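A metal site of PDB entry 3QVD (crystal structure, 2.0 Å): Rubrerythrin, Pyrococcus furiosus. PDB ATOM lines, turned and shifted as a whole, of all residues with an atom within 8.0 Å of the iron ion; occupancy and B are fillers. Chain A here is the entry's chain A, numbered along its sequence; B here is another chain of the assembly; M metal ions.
N of Val 158 lies close to SG of Cys 156 (3.4 Å). N of Cys 156 sits at hydrogen-bond distance from O of Ala 161. O of Tyr 146 is in hydrogen-bond range of N of Cys 141. SG of Cys 141 lies close to N of Ile 143. The side-chain sulfur of Cys 159 sits close to the backbone NH of Ala 161, 3.6 Å away. The backbone NH (N) of Tyr 146 sits close to the side-chain sulfur (SG) of Cys 144, 3.4 Å away.
Within 4 Å of the iron ion: Cys 141, Cys 144, Cys 156 and Cys 159. Along chain A the residues within 4 Å of the iron ion span positions 141 to 159.
The iron ion is bound by the side-chain sulfur (SG) of Cys 156 (2.3 Å), the side-chain sulfur (SG) of Cys 141 (2.3 Å), the side-chain sulfur (SG) of Cys 159 (2.3 Å) and the side-chain sulfur (SG) of Cys 144 (2.3 Å).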
ATOM      1  N   TYR A 108       1.349  18.527 -17.975  1.00  0.00           N
ATOM      2  CA  TYR A 108       1.672  17.686 -19.119  1.00  0.00           C
ATOM      3  C   TYR A 108       2.781  16.692 -18.766  1.00  0.00           C
ATOM      4  O   TYR A 108       2.634  15.485 -18.962  1.00  0.00           O
ATOM      5  CB  TYR A 108       2.146  18.538 -20.309  1.00  0.00           C
ATOM      6  CG  TYR A 108       1.052  19.205 -21.123  1.00  0.00           C
ATOM      7  CD1 TYR A 108      -0.299  19.008 -20.814  1.00  0.00           C
ATOM      8  CD2 TYR A 108       1.356  20.006 -22.224  1.00  0.00           C
ATOM      9  CE1 TYR A 108      -1.311  19.584 -21.581  1.00  0.00           C
ATOM     10  CE2 TYR A 108       0.352  20.592 -22.996  1.00  0.00           C
ATOM     11  CZ  TYR A 108      -0.976  20.370 -22.674  1.00  0.00           C
ATOM     12  OH  TYR A 108      -1.978  20.938 -23.437  1.00  0.00           O
ATOM     13  N   ILE A 140       4.322   8.562 -28.946  1.00  0.00           N
ATOM     14  CA  ILE A 140       4.601   9.692 -28.075  1.00  0.00           C
ATOM     15  C   ILE A 140       3.854  10.894 -28.629  1.00  0.00           C
ATOM     16  O   ILE A 140       3.970  11.200 -29.822  1.00  0.00           O
ATOM     17  CB  ILE A 140       6.113  10.065 -28.028  1.00  0.00           C
ATOM     18  CG1 ILE A 140       6.977   8.844 -27.705  1.00  0.00           C
ATOM     19  CG2 ILE A 140       6.329  11.147 -26.959  1.00  0.00           C
ATOM     20  CD1 ILE A 140       6.814   8.288 -26.308  1.00  0.00           C
ATOM     21  N   CYS A 141       3.092  11.569 -27.783  1.00  0.00           N
ATOM     22  CA  CYS A 141       2.363  12.753 -28.226  1.00  0.00           C
ATOM     23  C   CYS A 141       3.350  13.923 -28.303  1.00  0.00           C
ATOM     24  O   CYS A 141       4.013  14.245 -27.321  1.00  0.00           O
ATOM     25  CB  CYS A 141       1.228  13.061 -27.240  1.00  0.00           C
ATOM     26  SG  CYS A 141       0.297  14.566 -27.613  1.00  0.00           S
ATOM     27  N   PRO A 142       3.440  14.570 -29.474  1.00  0.00           N
ATOM     28  CA  PRO A 142       4.351  15.699 -29.675  1.00  0.00           C
ATOM     29  C   PRO A 142       3.938  16.957 -28.925  1.00  0.00           C
ATOM     30  O   PRO A 142       4.700  17.925 -28.842  1.00  0.00           O
ATOM     31  CB  PRO A 142       4.324  15.899 -31.183  1.00  0.00           C
ATOM     32  CG  PRO A 142       2.899  15.588 -31.515  1.00  0.00           C
ATOM     33  CD  PRO A 142       2.654  14.316 -30.706  1.00  0.00           C
ATOM     34  N   ILE A 143       2.741  16.942 -28.355  1.00  0.00           N
ATOM     35  CA  ILE A 143       2.235  18.089 -27.622  1.00  0.00           C
ATOM     36  C   ILE A 143       2.530  18.041 -26.124  1.00  0.00           C
ATOM     37  O   ILE A 143       3.043  19.011 -25.558  1.00  0.00           O
ATOM     38  CB  ILE A 143       0.701  18.239 -27.816  1.00  0.00           C
ATOM     39  CG1 ILE A 143       0.373  18.335 -29.304  1.00  0.00           C
ATOM     40  CG2 ILE A 143       0.187  19.479 -27.099  1.00  0.00           C
ATOM     41  CD1 ILE A 143       1.120  19.430 -30.041  1.00  0.00           C
ATOM     42  N   CYS A 144       2.231  16.921 -25.487  1.00  0.00           N
ATOM     43  CA  CYS A 144       2.419  16.781 -24.051  1.00  0.00           C
ATOM     44  C   CYS A 144       3.344  15.649 -23.618  1.00  0.00           C
ATOM     45  O   CYS A 144       3.599  15.476 -22.427  1.00  0.00           O
ATOM     46  CB  CYS A 144       1.053  16.571 -23.382  1.00  0.00           C
ATOM     47  SG  CYS A 144       0.354  14.949 -23.760  1.00  0.00           S
ATOM     48  N   GLY A 145       3.836  14.863 -24.569  1.00  0.00           N
ATOM     49  CA  GLY A 145       4.732  13.771 -24.225  1.00  0.00           C
ATOM     50  C   GLY A 145       4.031  12.511 -23.742  1.00  0.00           C
ATOM     51  O   GLY A 145       4.700  11.573 -23.295  1.00  0.00           O
ATOM     52  N   TYR A 146       2.702  12.484 -23.799  1.00  0.00           N
ATOM     53  CA  TYR A 146       1.972  11.287 -23.383  1.00  0.00           C
ATOM     54  C   TYR A 146       2.614  10.098 -24.096  1.00  0.00           C
ATOM     55  O   TYR A 146       2.948  10.189 -25.291  1.00  0.00           O
ATOM     56  CB  TYR A 146       0.481  11.395 -23.748  1.00  0.00           C
ATOM     57  CG  TYR A 146      -0.256  10.073 -23.731  1.00  0.00           C
ATOM     58  CD1 TYR A 146      -0.468   9.357 -24.908  1.00  0.00           C
ATOM     59  CD2 TYR A 146      -0.724   9.522 -22.534  1.00  0.00           C
ATOM     60  CE1 TYR A 146      -1.134   8.139 -24.904  1.00  0.00           C
ATOM     61  CE2 TYR A 146      -1.399   8.300 -22.516  1.00  0.00           C
ATOM     62  CZ  TYR A 146      -1.595   7.620 -23.713  1.00  0.00           C
ATOM     63  OH  TYR A 146      -2.252   6.412 -23.714  1.00  0.00           O
ATOM     64  N   THR A 147       2.771   8.991 -23.386  1.00  0.00           N
ATOM     65  CA  THR A 147       3.433   7.809 -23.922  1.00  0.00           C
ATOM     66  C   THR A 147       2.562   6.558 -23.872  1.00  0.00           C
ATOM     67  O   THR A 147       1.907   6.291 -22.870  1.00  0.00           O
ATOM     68  CB  THR A 147       4.733   7.563 -23.136  1.00  0.00           C
ATOM     69  OG1 THR A 147       5.549   8.751 -23.185  1.00  0.00           O
ATOM     70  CG2 THR A 147       5.512   6.398 -23.706  1.00  0.00           C
ATOM     71  N   TYR A 155      -7.358   9.406 -29.085  1.00  0.00           N
ATOM     72  CA  TYR A 155      -7.018  10.794 -28.788  1.00  0.00           C
ATOM     73  C   TYR A 155      -6.179  10.806 -27.506  1.00  0.00           C
ATOM     74  O   TYR A 155      -6.436  10.013 -26.592  1.00  0.00           O
ATOM     75  CB  TYR A 155      -8.297  11.610 -28.586  1.00  0.00           C
ATOM     76  CG  TYR A 155      -9.136  11.750 -29.837  1.00  0.00           C
ATOM     77  CD1 TYR A 155      -8.783  12.644 -30.841  1.00  0.00           C
ATOM     78  CD2 TYR A 155     -10.272  10.950 -30.037  1.00  0.00           C
ATOM     79  CE1 TYR A 155      -9.513  12.733 -32.021  1.00  0.00           C
ATOM     80  CE2 TYR A 155     -11.012  11.039 -31.216  1.00  0.00           C
ATOM     81  CZ  TYR A 155     -10.627  11.935 -32.200  1.00  0.00           C
ATOM     82  OH  TYR A 155     -11.356  12.015 -33.376  1.00  0.00           O
ATOM     83  N   CYS A 156      -5.180  11.680 -27.457  1.00  0.00           N
ATOM     84  CA  CYS A 156      -4.334  11.786 -26.259  1.00  0.00           C
ATOM     85  C   CYS A 156      -5.217  12.134 -25.062  1.00  0.00           C
ATOM     86  O   CYS A 156      -5.962  13.113 -25.097  1.00  0.00           O
ATOM     87  CB  CYS A 156      -3.268  12.869 -26.451  1.00  0.00           C
ATOM     88  SG  CYS A 156      -2.254  13.127 -24.964  1.00  0.00           S
ATOM     89  N   PRO A 157      -5.132  11.360 -23.974  1.00  0.00           N
ATOM     90  CA  PRO A 157      -5.947  11.615 -22.773  1.00  0.00           C
ATOM     91  C   PRO A 157      -5.564  12.872 -22.007  1.00  0.00           C
ATOM     92  O   PRO A 157      -6.329  13.337 -21.149  1.00  0.00           O
ATOM     93  CB  PRO A 157      -5.729  10.351 -21.945  1.00  0.00           C
ATOM     94  CG  PRO A 157      -4.312   9.983 -22.257  1.00  0.00           C
ATOM     95  CD  PRO A 157      -4.241  10.201 -23.776  1.00  0.00           C
ATOM     96  N   VAL A 158      -4.403  13.431 -22.303  1.00  0.00           N
ATOM     97  CA  VAL A 158      -3.960  14.633 -21.611  1.00  0.00           C
ATOM     98  C   VAL A 158      -4.305  15.916 -22.355  1.00  0.00           C
ATOM     99  O   VAL A 158      -4.912  16.821 -21.773  1.00  0.00           O
ATOM    100  CB  VAL A 158      -2.432  14.601 -21.345  1.00  0.00           C
ATOM    101  CG1 VAL A 158      -2.002  15.870 -20.609  1.00  0.00           C
ATOM    102  CG2 VAL A 158      -2.057  13.367 -20.537  1.00  0.00           C
ATOM    103  N   CYS A 159      -3.945  15.998 -23.637  1.00  0.00           N
ATOM    104  CA  CYS A 159      -4.226  17.195 -24.427  1.00  0.00           C
ATOM    105  C   CYS A 159      -5.288  16.999 -25.513  1.00  0.00           C
ATOM    106  O   CYS A 159      -5.749  17.967 -26.118  1.00  0.00           O
ATOM    107  CB  CYS A 159      -2.943  17.718 -25.070  1.00  0.00           C
ATOM    108  SG  CYS A 159      -2.253  16.673 -26.374  1.00  0.00           S
ATOM    109  N   GLY A 160      -5.647  15.740 -25.778  1.00  0.00           N
ATOM    110  CA  GLY A 160      -6.667  15.474 -26.771  1.00  0.00           C
ATOM    111  C   GLY A 160      -6.229  15.436 -28.228  1.00  0.00           C
ATOM    112  O   GLY A 160      -7.067  15.359 -29.122  1.00  0.00           O
ATOM    113  N   ALA A 161      -4.923  15.492 -28.471  1.00  0.00           N
ATOM    114  CA  ALA A 161      -4.407  15.446 -29.834  1.00  0.00           C
ATOM    115  C   ALA A 161      -4.776  14.117 -30.482  1.00  0.00           C
ATOM    116  O   ALA A 161      -4.778  13.081 -29.818  1.00  0.00           O
ATOM    117  CB  ALA A 161      -2.891  15.612 -29.812  1.00  0.00           C
ATOM    118  N   PRO A 162      -5.105  14.132 -31.779  1.00  0.00           N
ATOM    119  CA  PRO A 162      -5.473  12.888 -32.461  1.00  0.00           C
ATOM    120  C   PRO A 162      -4.281  11.949 -32.618  1.00  0.00           C
ATOM    121  O   PRO A 162      -3.140  12.394 -32.760  1.00  0.00           O
ATOM    122  CB  PRO A 162      -6.025  13.377 -33.806  1.00  0.00           C
ATOM    123  CG  PRO A 162      -5.227  14.617 -34.053  1.00  0.00           C
ATOM    124  CD  PRO A 162      -5.240  15.288 -32.699  1.00  0.00           C
ATOM    125  N   PHE A 166       0.732  11.376 -33.221  1.00  0.00           N
ATOM    126  CA  PHE A 166       1.708  10.715 -32.350  1.00  0.00           C
ATOM    127  C   PHE A 166       2.976  10.312 -33.118  1.00  0.00           C
ATOM    128  O   PHE A 166       2.902   9.802 -34.238  1.00  0.00           O
ATOM    129  CB  PHE A 166       1.119   9.450 -31.708  1.00  0.00           C
ATOM    130  CG  PHE A 166      -0.045   9.700 -30.781  1.00  0.00           C
ATOM    131  CD1 PHE A 166      -0.439  10.997 -30.451  1.00  0.00           C
ATOM    132  CD2 PHE A 166      -0.736   8.631 -30.220  1.00  0.00           C
ATOM    133  CE1 PHE A 166      -1.513  11.213 -29.564  1.00  0.00           C
ATOM    134  CE2 PHE A 166      -1.799   8.829 -29.347  1.00  0.00           C
ATOM    135  CZ  PHE A 166      -2.182  10.118 -29.012  1.00  0.00           C
ATOM    136  N   VAL B  53       9.845  16.784 -25.614  1.00  0.00           N
ATOM    137  CA  VAL B  53       8.584  17.517 -25.697  1.00  0.00           C
ATOM    138  C   VAL B  53       8.404  18.325 -24.413  1.00  0.00           C
ATOM    139  O   VAL B  53       8.083  19.518 -24.460  1.00  0.00           O
ATOM    140  CB  VAL B  53       7.394  16.547 -25.860  1.00  0.00           C
ATOM    141  CG1 VAL B  53       6.083  17.313 -25.744  1.00  0.00           C
ATOM    142  CG2 VAL B  53       7.469  15.858 -27.218  1.00  0.00           C
HETATM  143 FE    FE M   1      -0.965  14.864 -25.686  1.00  0.00          FE
